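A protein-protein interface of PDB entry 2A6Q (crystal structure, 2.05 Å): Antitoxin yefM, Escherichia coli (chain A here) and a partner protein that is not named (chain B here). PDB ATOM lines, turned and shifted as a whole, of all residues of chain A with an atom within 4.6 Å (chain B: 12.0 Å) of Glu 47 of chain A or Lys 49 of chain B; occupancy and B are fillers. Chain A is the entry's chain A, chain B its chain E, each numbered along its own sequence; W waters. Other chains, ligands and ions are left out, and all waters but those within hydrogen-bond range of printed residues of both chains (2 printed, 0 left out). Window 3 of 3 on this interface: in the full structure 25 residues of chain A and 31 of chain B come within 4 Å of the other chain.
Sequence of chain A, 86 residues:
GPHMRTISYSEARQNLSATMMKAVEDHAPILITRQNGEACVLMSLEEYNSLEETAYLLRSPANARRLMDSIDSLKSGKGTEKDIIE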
ATOM      1  N   HIS A  27      11.460  26.404 -33.210  1.00  0.00           N
ATOM      2  CA  HIS A  27      11.605  25.695 -31.942  1.00  0.00           C
ATOM      3  C   HIS A  27      11.110  24.270 -32.107  1.00  0.00           C
ATOM      4  O   HIS A  27      10.554  23.667 -31.185  1.00  0.00           O
ATOM      5  CB  HIS A  27      10.814  26.390 -30.839  1.00  0.00           C
ATOM      6  CG  HIS A  27      11.391  27.706 -30.427  1.00  0.00           C
ATOM      7  ND1 HIS A  27      11.333  28.828 -31.226  1.00  0.00           N
ATOM      8  CD2 HIS A  27      12.072  28.070 -29.314  1.00  0.00           C
ATOM      9  CE1 HIS A  27      11.954  29.828 -30.622  1.00  0.00           C
ATOM     10  NE2 HIS A  27      12.411  29.394 -29.462  1.00  0.00           N
ATOM     11  N   MET A  43      18.110  19.909 -33.590  1.00  0.00           N
ATOM     12  CA  MET A  43      17.233  20.846 -32.901  1.00  0.00           C
ATOM     13  C   MET A  43      18.055  22.032 -32.449  1.00  0.00           C
ATOM     14  O   MET A  43      19.283  21.945 -32.363  1.00  0.00           O
ATOM     15  CB  MET A  43      16.556  20.180 -31.695  1.00  0.00           C
ATOM     16  CG  MET A  43      17.506  19.705 -30.597  1.00  0.00           C
ATOM     17  SD  MET A  43      16.610  18.900 -29.237  1.00  0.00           S
ATOM     18  CE  MET A  43      16.549  17.276 -29.771  1.00  0.00           C
ATOM     19  N   SER A  44      17.384  23.143 -32.168  1.00  0.00           N
ATOM     20  CA  SER A  44      18.080  24.340 -31.712  1.00  0.00           C
ATOM     21  C   SER A  44      18.700  24.072 -30.336  1.00  0.00           C
ATOM     22  O   SER A  44      18.207  23.228 -29.580  1.00  0.00           O
ATOM     23  CB  SER A  44      17.103  25.515 -31.625  1.00  0.00           C
ATOM     24  OG  SER A  44      16.203  25.344 -30.546  1.00  0.00           O
ATOM     25  N   LEU A  45      19.783  24.777 -30.017  1.00  0.00           N
ATOM     26  CA  LEU A  45      20.443  24.597 -28.726  1.00  0.00           C
ATOM     27  C   LEU A  45      19.454  24.890 -27.605  1.00  0.00           C
ATOM     28  O   LEU A  45      19.413  24.200 -26.588  1.00  0.00           O
ATOM     29  CB  LEU A  45      21.645  25.539 -28.595  1.00  0.00           C
ATOM     30  CG  LEU A  45      22.383  25.471 -27.250  1.00  0.00           C
ATOM     31  CD1 LEU A  45      22.839  24.042 -26.957  1.00  0.00           C
ATOM     32  CD2 LEU A  45      23.576  26.420 -27.290  1.00  0.00           C
ATOM     33  N   GLU A  46      18.668  25.937 -27.813  1.00  0.00           N
ATOM     34  CA  GLU A  46      17.660  26.370 -26.857  1.00  0.00           C
ATOM     35  C   GLU A  46      16.663  25.253 -26.559  1.00  0.00           C
ATOM     36  O   GLU A  46      16.335  24.989 -25.404  1.00  0.00           O
ATOM     37  CB  GLU A  46      16.937  27.585 -27.436  1.00  0.00           C
ATOM     38  CG  GLU A  46      15.800  28.121 -26.600  1.00  0.00           C
ATOM     39  CD  GLU A  46      15.151  29.324 -27.258  1.00  0.00           C
ATOM     40  OE1 GLU A  46      14.271  29.944 -26.631  1.00  0.00           O
ATOM     41  OE2 GLU A  46      15.528  29.643 -28.410  1.00  0.00           O
ATOM     42  N   GLU A  47      16.183  24.589 -27.602  1.00  0.00           N
ATOM     43  CA  GLU A  47      15.229  23.510 -27.398  1.00  0.00           C
ATOM     44  C   GLU A  47      15.908  22.317 -26.745  1.00  0.00           C
ATOM     45  O   GLU A  47      15.313  21.644 -25.906  1.00  0.00           O
ATOM     46  CB  GLU A  47      14.577  23.114 -28.727  1.00  0.00           C
ATOM     47  CG  GLU A  47      13.495  24.104 -29.173  1.00  0.00           C
ATOM     48  CD  GLU A  47      12.336  24.195 -28.175  1.00  0.00           C
ATOM     49  OE1 GLU A  47      11.711  23.146 -27.912  1.00  0.00           O
ATOM     50  OE2 GLU A  47      12.056  25.303 -27.657  1.00  0.00           O
ATOM     51  N   TYR A  48      17.156  22.056 -27.123  1.00  0.00           N
ATOM     52  CA  TYR A  48      17.881  20.950 -26.521  1.00  0.00           C
ATOM     53  C   TYR A  48      18.064  21.180 -25.017  1.00  0.00           C
ATOM     54  O   TYR A  48      17.801  20.295 -24.212  1.00  0.00           O
ATOM     55  CB  TYR A  48      19.257  20.770 -27.170  1.00  0.00           C
ATOM     56  CG  TYR A  48      20.086  19.740 -26.445  1.00  0.00           C
ATOM     57  CD1 TYR A  48      19.788  18.383 -26.545  1.00  0.00           C
ATOM     58  CD2 TYR A  48      21.103  20.130 -25.576  1.00  0.00           C
ATOM     59  CE1 TYR A  48      20.476  17.436 -25.788  1.00  0.00           C
ATOM     60  CE2 TYR A  48      21.800  19.188 -24.814  1.00  0.00           C
ATOM     61  CZ  TYR A  48      21.477  17.847 -24.923  1.00  0.00           C
ATOM     62  OH  TYR A  48      22.130  16.921 -24.142  1.00  0.00           O
ATOM     63  N   ASN A  49      18.532  22.367 -24.647  1.00  0.00           N
ATOM     64  CA  ASN A  49      18.751  22.696 -23.244  1.00  0.00           C
ATOM     65  C   ASN A  49      17.460  22.560 -22.429  1.00  0.00           C
ATOM     66  O   ASN A  49      17.483  22.116 -21.279  1.00  0.00           O
ATOM     67  CB  ASN A  49      19.315  24.121 -23.124  1.00  0.00           C
ATOM     68  CG  ASN A  49      20.796  24.203 -23.512  1.00  0.00           C
ATOM     69  OD1 ASN A  49      21.325  25.284 -23.774  1.00  0.00           O
ATOM     70  ND2 ASN A  49      21.466  23.055 -23.539  1.00  0.00           N
ATOM     71  N   SER A  50      16.335  22.931 -23.032  1.00  0.00           N
ATOM     72  CA  SER A  50      15.054  22.834 -22.340  1.00  0.00           C
ATOM     73  C   SER A  50      14.681  21.374 -22.104  1.00  0.00           C
ATOM     74  O   SER A  50      14.310  20.993 -20.999  1.00  0.00           O
ATOM     75  CB  SER A  50      13.946  23.522 -23.147  1.00  0.00           C
ATOM     76  OG  SER A  50      12.680  23.254 -22.562  1.00  0.00           O
ATOM     77  N   LEU A  51      14.789  20.558 -23.144  1.00  0.00           N
ATOM     78  CA  LEU A  51      14.460  19.146 -23.031  1.00  0.00           C
ATOM     79  C   LEU A  51      15.373  18.408 -22.057  1.00  0.00           C
ATOM     80  O   LEU A  51      14.910  17.588 -21.271  1.00  0.00           O
ATOM     81  CB  LEU A  51      14.531  18.471 -24.405  1.00  0.00           C
ATOM     82  CG  LEU A  51      14.401  16.941 -24.422  1.00  0.00           C
ATOM     83  CD1 LEU A  51      13.038  16.527 -23.866  1.00  0.00           C
ATOM     84  CD2 LEU A  51      14.579  16.418 -25.848  1.00  0.00           C
ATOM     85  N   THR A  54      14.637  19.256 -18.407  1.00  0.00           N
ATOM     86  CA  THR A  54      13.365  18.661 -18.000  1.00  0.00           C
ATOM     87  C   THR A  54      13.580  17.194 -17.660  1.00  0.00           C
ATOM     88  O   THR A  54      13.077  16.686 -16.649  1.00  0.00           O
ATOM     89  CB  THR A  54      12.299  18.740 -19.137  1.00  0.00           C
ATOM     90  OG1 THR A  54      12.065  20.110 -19.486  1.00  0.00           O
ATOM     91  CG2 THR A  54      10.983  18.116 -18.685  1.00  0.00           C
ATOM     92  N   LYS B  44      21.344  30.485 -15.229  1.00  0.00           N
ATOM     93  CA  LYS B  44      21.018  29.945 -16.542  1.00  0.00           C
ATOM     94  C   LYS B  44      19.565  29.467 -16.567  1.00  0.00           C
ATOM     95  O   LYS B  44      19.292  28.267 -16.652  1.00  0.00           O
ATOM     96  CB  LYS B  44      21.968  28.783 -16.869  1.00  0.00           C
ATOM     97  CG  LYS B  44      21.928  28.304 -18.317  1.00  0.00           C
ATOM     98  CD  LYS B  44      22.736  27.018 -18.505  1.00  0.00           C
ATOM     99  CE  LYS B  44      24.234  27.219 -18.268  1.00  0.00           C
ATOM    100  NZ  LYS B  44      24.895  28.049 -19.319  1.00  0.00           N
ATOM    101  N   PRO B  45      18.611  30.410 -16.479  1.00  0.00           N
ATOM    102  CA  PRO B  45      17.176  30.114 -16.489  1.00  0.00           C
ATOM    103  C   PRO B  45      16.769  29.243 -17.674  1.00  0.00           C
ATOM    104  O   PRO B  45      17.105  29.539 -18.817  1.00  0.00           O
ATOM    105  CB  PRO B  45      16.543  31.501 -16.550  1.00  0.00           C
ATOM    106  CG  PRO B  45      17.511  32.336 -15.772  1.00  0.00           C
ATOM    107  CD  PRO B  45      18.846  31.853 -16.290  1.00  0.00           C
ATOM    108  N   GLU B  46      16.027  28.179 -17.403  1.00  0.00           N
ATOM    109  CA  GLU B  46      15.606  27.281 -18.461  1.00  0.00           C
ATOM    110  C   GLU B  46      14.128  26.900 -18.371  1.00  0.00           C
ATOM    111  O   GLU B  46      13.656  26.463 -17.323  1.00  0.00           O
ATOM    112  CB  GLU B  46      16.457  26.007 -18.417  1.00  0.00           C
ATOM    113  CG  GLU B  46      16.630  25.331 -19.756  1.00  0.00           C
ATOM    114  CD  GLU B  46      17.524  26.120 -20.685  1.00  0.00           C
ATOM    115  OE1 GLU B  46      18.703  26.337 -20.334  1.00  0.00           O
ATOM    116  OE2 GLU B  46      17.049  26.524 -21.766  1.00  0.00           O
ATOM    117  N   PRO B  47      13.380  27.063 -19.475  1.00  0.00           N
ATOM    118  CA  PRO B  47      11.957  26.722 -19.509  1.00  0.00           C
ATOM    119  C   PRO B  47      11.806  25.204 -19.606  1.00  0.00           C
ATOM    120  O   PRO B  47      12.550  24.548 -20.344  1.00  0.00           O
ATOM    121  CB  PRO B  47      11.465  27.440 -20.760  1.00  0.00           C
ATOM    122  CG  PRO B  47      12.654  27.337 -21.676  1.00  0.00           C
ATOM    123  CD  PRO B  47      13.802  27.685 -20.744  1.00  0.00           C
ATOM    124  N   LEU B  48      10.849  24.648 -18.868  1.00  0.00           N
ATOM    125  CA  LEU B  48      10.635  23.205 -18.857  1.00  0.00           C
ATOM    126  C   LEU B  48       9.531  22.736 -19.807  1.00  0.00           C
ATOM    127  O   LEU B  48       8.646  23.501 -20.184  1.00  0.00           O
ATOM    128  CB  LEU B  48      10.359  22.749 -17.418  1.00  0.00           C
ATOM    129  CG  LEU B  48      11.432  23.258 -16.435  1.00  0.00           C
ATOM    130  CD1 LEU B  48      11.098  22.823 -15.002  1.00  0.00           C
ATOM    131  CD2 LEU B  48      12.802  22.716 -16.847  1.00  0.00           C
ATOM    132  N   LYS B  49       9.591  21.466 -20.188  1.00  0.00           N
ATOM    133  CA  LYS B  49       8.632  20.906 -21.130  1.00  0.00           C
ATOM    134  C   LYS B  49       7.653  19.865 -20.587  1.00  0.00           C
ATOM    135  O   LYS B  49       7.746  19.412 -19.439  1.00  0.00           O
ATOM    136  CB  LYS B  49       9.388  20.274 -22.300  1.00  0.00           C
ATOM    137  CG  LYS B  49      10.244  21.225 -23.108  1.00  0.00           C
ATOM    138  CD  LYS B  49      10.909  20.468 -24.252  1.00  0.00           C
ATOM    139  CE  LYS B  49      11.617  21.413 -25.208  1.00  0.00           C
ATOM    140  NZ  LYS B  49      10.670  22.438 -25.715  1.00  0.00           N
ATOM    141  N   HIS B  50       6.720  19.486 -21.459  1.00  0.00           N
ATOM    142  CA  HIS B  50       5.702  18.480 -21.172  1.00  0.00           C
ATOM    143  C   HIS B  50       5.032  18.700 -19.827  1.00  0.00           C
ATOM    144  O   HIS B  50       4.650  19.821 -19.502  1.00  0.00           O
ATOM    145  CB  HIS B  50       6.327  17.082 -21.240  1.00  0.00           C
ATOM    146  CG  HIS B  50       7.108  16.837 -22.496  1.00  0.00           C
ATOM    147  ND1 HIS B  50       6.591  17.074 -23.753  1.00  0.00           N
ATOM    148  CD2 HIS B  50       8.373  16.396 -22.690  1.00  0.00           C
ATOM    149  CE1 HIS B  50       7.504  16.794 -24.665  1.00  0.00           C
ATOM    150  NE2 HIS B  50       8.596  16.380 -24.046  1.00  0.00           N
ATOM    151  N   ASN B  51       4.904  17.639 -19.037  1.00  0.00           N
ATOM    152  CA  ASN B  51       4.256  17.750 -17.733  1.00  0.00           C
ATOM    153  C   ASN B  51       4.765  18.915 -16.877  1.00  0.00           C
ATOM    154  O   ASN B  51       4.089  19.334 -15.939  1.00  0.00           O
ATOM    155  CB  ASN B  51       4.378  16.424 -16.969  1.00  0.00           C
ATOM    156  CG  ASN B  51       3.657  15.278 -17.674  1.00  0.00           C
ATOM    157  OD1 ASN B  51       2.442  15.326 -17.882  1.00  0.00           O
ATOM    158  ND2 ASN B  51       4.405  14.243 -18.046  1.00  0.00           N
ATOM    159  N   LEU B  52       5.941  19.450 -17.204  1.00  0.00           N
ATOM    160  CA  LEU B  52       6.495  20.577 -16.446  1.00  0.00           C
ATOM    161  C   LEU B  52       6.299  21.912 -17.161  1.00  0.00           C
ATOM    162  O   LEU B  52       6.828  22.932 -16.730  1.00  0.00           O
ATOM    163  CB  LEU B  52       7.994  20.374 -16.191  1.00  0.00           C
ATOM    164  CG  LEU B  52       8.411  19.219 -15.279  1.00  0.00           C
ATOM    165  CD1 LEU B  52       9.925  19.264 -15.044  1.00  0.00           C
ATOM    166  CD2 LEU B  52       7.669  19.328 -13.952  1.00  0.00           C
ATOM    167  N   SER B  53       5.545  21.905 -18.255  1.00  0.00           N
ATOM    168  CA  SER B  53       5.314  23.132 -19.008  1.00  0.00           C
ATOM    169  C   SER B  53       4.874  24.256 -18.093  1.00  0.00           C
ATOM    170  O   SER B  53       4.075  24.049 -17.182  1.00  0.00           O
ATOM    171  CB  SER B  53       4.256  22.910 -20.089  1.00  0.00           C
ATOM    172  OG  SER B  53       4.745  22.036 -21.084  1.00  0.00           O
ATOM    173  N   GLY B  54       5.400  25.448 -18.338  1.00  0.00           N
ATOM    174  CA  GLY B  54       5.040  26.585 -17.518  1.00  0.00           C
ATOM    175  C   GLY B  54       6.062  26.847 -16.433  1.00  0.00           C
ATOM    176  O   GLY B  54       6.166  27.964 -15.928  1.00  0.00           O
ATOM    177  N   PHE B  55       6.817  25.821 -16.055  1.00  0.00           N
ATOM    178  CA  PHE B  55       7.821  26.017 -15.022  1.00  0.00           C
ATOM    179  C   PHE B  55       9.214  26.241 -15.578  1.00  0.00           C
ATOM    180  O   PHE B  55       9.501  25.894 -16.726  1.00  0.00           O
ATOM    181  CB  PHE B  55       7.814  24.855 -14.030  1.00  0.00           C
ATOM    182  CG  PHE B  55       6.737  24.972 -12.998  1.00  0.00           C
ATOM    183  CD1 PHE B  55       5.406  24.726 -13.331  1.00  0.00           C
ATOM    184  CD2 PHE B  55       7.042  25.376 -11.701  1.00  0.00           C
ATOM    185  CE1 PHE B  55       4.397  24.883 -12.389  1.00  0.00           C
ATOM    186  CE2 PHE B  55       6.039  25.538 -10.751  1.00  0.00           C
ATOM    187  CZ  PHE B  55       4.710  25.289 -11.098  1.00  0.00           C
ATOM    188  N   TRP B  56      10.060  26.840 -14.746  1.00  0.00           N
ATOM    189  CA  TRP B  56      11.433  27.174 -15.097  1.00  0.00           C
ATOM    190  C   TRP B  56      12.424  26.618 -14.085  1.00  0.00           C
ATOM    191  O   TRP B  56      12.065  26.321 -12.944  1.00  0.00           O
ATOM    192  CB  TRP B  56      11.592  28.693 -15.175  1.00  0.00           C
ATOM    193  CG  TRP B  56      10.878  29.305 -16.339  1.00  0.00           C
ATOM    194  CD1 TRP B  56       9.527  29.357 -16.542  1.00  0.00           C
ATOM    195  CD2 TRP B  56      11.481  29.906 -17.489  1.00  0.00           C
ATOM    196  NE1 TRP B  56       9.252  29.951 -17.753  1.00  0.00           N
ATOM    197  CE2 TRP B  56      10.434  30.299 -18.354  1.00  0.00           C
ATOM    198  CE3 TRP B  56      12.808  30.150 -17.875  1.00  0.00           C
ATOM    199  CZ2 TRP B  56      10.673  30.922 -19.585  1.00  0.00           C
ATOM    200  CZ3 TRP B  56      13.047  30.769 -19.100  1.00  0.00           C
ATOM    201  CH2 TRP B  56      11.981  31.149 -19.940  1.00  0.00           C
ATOM    202  N   SER B  57      13.679  26.499 -14.506  1.00  0.00           N
ATOM    203  CA  SER B  57      14.724  25.967 -13.646  1.00  0.00           C
ATOM    204  C   SER B  57      16.013  26.782 -13.675  1.00  0.00           C
ATOM    205  O   SER B  57      16.508  27.143 -14.745  1.00  0.00           O
ATOM    206  CB  SER B  57      15.027  24.517 -14.050  1.00  0.00           C
ATOM    207  OG  SER B  57      16.106  23.983 -13.302  1.00  0.00           O
ATOM    208  N   ARG B  58      16.547  27.078 -12.495  1.00  0.00           N
ATOM    209  CA  ARG B  58      17.805  27.808 -12.376  1.00  0.00           C
ATOM    210  C   ARG B  58      18.766  27.012 -11.498  1.00  0.00           C
ATOM    211  O   ARG B  58      18.345  26.268 -10.607  1.00  0.00           O
ATOM    212  CB  ARG B  58      17.593  29.196 -11.782  1.00  0.00           C
ATOM    213  CG  ARG B  58      16.865  30.149 -12.705  1.00  0.00           C
ATOM    214  CD  ARG B  58      16.961  31.570 -12.189  1.00  0.00           C
ATOM    215  NE  ARG B  58      16.094  32.492 -12.919  1.00  0.00           N
ATOM    216  CZ  ARG B  58      16.313  33.800 -13.000  1.00  0.00           C
ATOM    217  NH1 ARG B  58      17.373  34.327 -12.402  1.00  0.00           N
ATOM    218  NH2 ARG B  58      15.466  34.581 -13.662  1.00  0.00           N
ATOM    219  N   VAL B  67      13.278  25.477  -8.975  1.00  0.00           N
ATOM    220  CA  VAL B  67      12.230  25.270  -9.966  1.00  0.00           C
ATOM    221  C   VAL B  67      11.080  26.204  -9.605  1.00  0.00           C
ATOM    222  O   VAL B  67      10.694  26.304  -8.438  1.00  0.00           O
ATOM    223  CB  VAL B  67      11.755  23.806  -9.965  1.00  0.00           C
ATOM    224  CG1 VAL B  67      10.744  23.577 -11.092  1.00  0.00           C
ATOM    225  CG2 VAL B  67      12.965  22.880 -10.138  1.00  0.00           C
ATOM    226  N   TYR B  68      10.523  26.884 -10.602  1.00  0.00           N
ATOM    227  CA  TYR B  68       9.459  27.845 -10.326  1.00  0.00           C
ATOM    228  C   TYR B  68       8.611  28.209 -11.542  1.00  0.00           C
ATOM    229  O   TYR B  68       8.990  27.957 -12.688  1.00  0.00           O
ATOM    230  CB  TYR B  68      10.097  29.124  -9.781  1.00  0.00           C
ATOM    231  CG  TYR B  68      10.964  29.808 -10.817  1.00  0.00           C
ATOM    232  CD1 TYR B  68      10.403  30.661 -11.770  1.00  0.00           C
ATOM    233  CD2 TYR B  68      12.338  29.560 -10.882  1.00  0.00           C
ATOM    234  CE1 TYR B  68      11.183  31.251 -12.759  1.00  0.00           C
ATOM    235  CE2 TYR B  68      13.130  30.147 -11.870  1.00  0.00           C
ATOM    236  CZ  TYR B  68      12.546  30.993 -12.806  1.00  0.00           C
ATOM    237  OH  TYR B  68      13.318  31.583 -13.784  1.00  0.00           O
ATOM    238  N   ALA B  69       7.462  28.818 -11.270  1.00  0.00           N
ATOM    239  CA  ALA B  69       6.554  29.275 -12.311  1.00  0.00           C
ATOM    240  C   ALA B  69       6.218  30.721 -11.965  1.00  0.00           C
ATOM    241  O   ALA B  69       6.479  31.179 -10.850  1.00  0.00           O
ATOM    242  CB  ALA B  69       5.296  28.428 -12.338  1.00  0.00           C
HETATM  243  O   HOH W   1      10.871  24.607 -24.120  1.00  0.00           O
HETATM  244  O   HOH W   2      19.396  28.096 -23.780  1.00  0.00           O
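Among the printed residues, merely in contact across the chains: Ser 50 of chain A with Lys 49 of chain B (3.2 Å), Thr 54 of chain A with Leu 48 of chain B (3.5 Å), Asn 49 of chain A with Glu 46 of chain B (3.6 Å), Ser 50 of chain A with Glu 46 of chain B (3.9 Å), Leu 51 of chain A with Lys 49 of chain B (3.9 Å) and Thr 54 of chain A with Leu 52 of chain B (3.96 Å).
The side-chain amino group (NZ) of Lys 49 of chain B is in salt-bridge range of the side-chain carboxylate (OE1) of Glu 47 of chain A, at 2.5 Å.
The backbone carbonyl oxygen (O) of Pro 47 of chain B sits at hydrogen-bond distance from the side-chain hydroxyl (OG) of Ser 50 of chain A (2.6 Å).
The side-chain hydroxyl (OG1) of Thr 54 of chain A sits at hydrogen-bond distance from the backbone NH (N) of Lys 49 of chain B (2.9 Å).
Lys 49 of chain B touches just these residues of chain A: Glu 47, Ser 50, Leu 51 and Thr 54.
No residue of chain B comes within 4 Å of His 27 of chain A.
No residue of chain B comes within 4 Å of Leu 45 of chain A.
Of the printed residues of chain B, Asn 49 of chain A touches Glu 46.
Of chain B, only Glu 46 (3.9 Å), Pro 47 (2.6 Å) and Lys 49 (3.2 Å) come within 4 Å of Ser 50 of chain A.
Leu 51 of chain A touches just one residue of chain B: Lys 49.
Of chain B, only Leu 48, Lys 49 and Leu 52 come within 4 Å of Thr 54 of chain A.
Of the printed residues of chain A, Leu 48 of chain B touches Thr 54 (3.5 Å).
Of the printed residues of chain A, Glu 46 of chain B touches Asn 49 and Ser 50.
Of the printed residues of chain A, Leu 52 of chain B touches Thr 54 (3.96 Å).
Glu 46 of chain A touches none of the printed residues of chain B.
The nearest residue of chain B that does not touch Glu 47 of chain A is Glu 46 of chain B (6.2 Å).
The nearest printed residue of chain A that does not touch Lys 49 of chain B is His 27 of chain A (5.6 Å).
The nearest printed residue of chain A that does not touch Glu 46 of chain B is Glu 46 of chain A (4.01 Å).
The side-chain hydroxyl of Ser 44 of chain A lies within hydrogen-bond range of the backbone NH of Glu 47 of chain A (3.0 Å).
The side-chain hydroxyl (OG1) of Thr 54 of chain A is in hydrogen-bond range of the backbone carbonyl oxygen (O) of Ser 50 of chain A (2.8 Å).
The backbone carbonyl oxygen (O) of Glu 46 of chain B sits at hydrogen-bond distance from the backbone NH (N) of Ser 57 of chain B (2.8 Å).
The backbone NH (N) of Leu 48 of chain B lies within hydrogen-bond range of the backbone carbonyl oxygen (O) of Phe 55 of chain B.
Water W1 lies within hydrogen-bond range of the side-chain amino group of Lys 49 of chain B (2.7 Å) and the side-chain hydroxyl of Ser 50 of chain A (2.7 Å).
Water W2 bridges OD1 of Asn 49 of chain A (3.4 Å) and OE2 of Glu 46 of chain B (3.5 Å).
Hydrophobic or aromatic side chains of chain B within 4 Å of the printed part of chain A: Leu 48 and Leu 52.
Of the 11 printed residues of chain A, 5 touch a printed residue of chain B.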
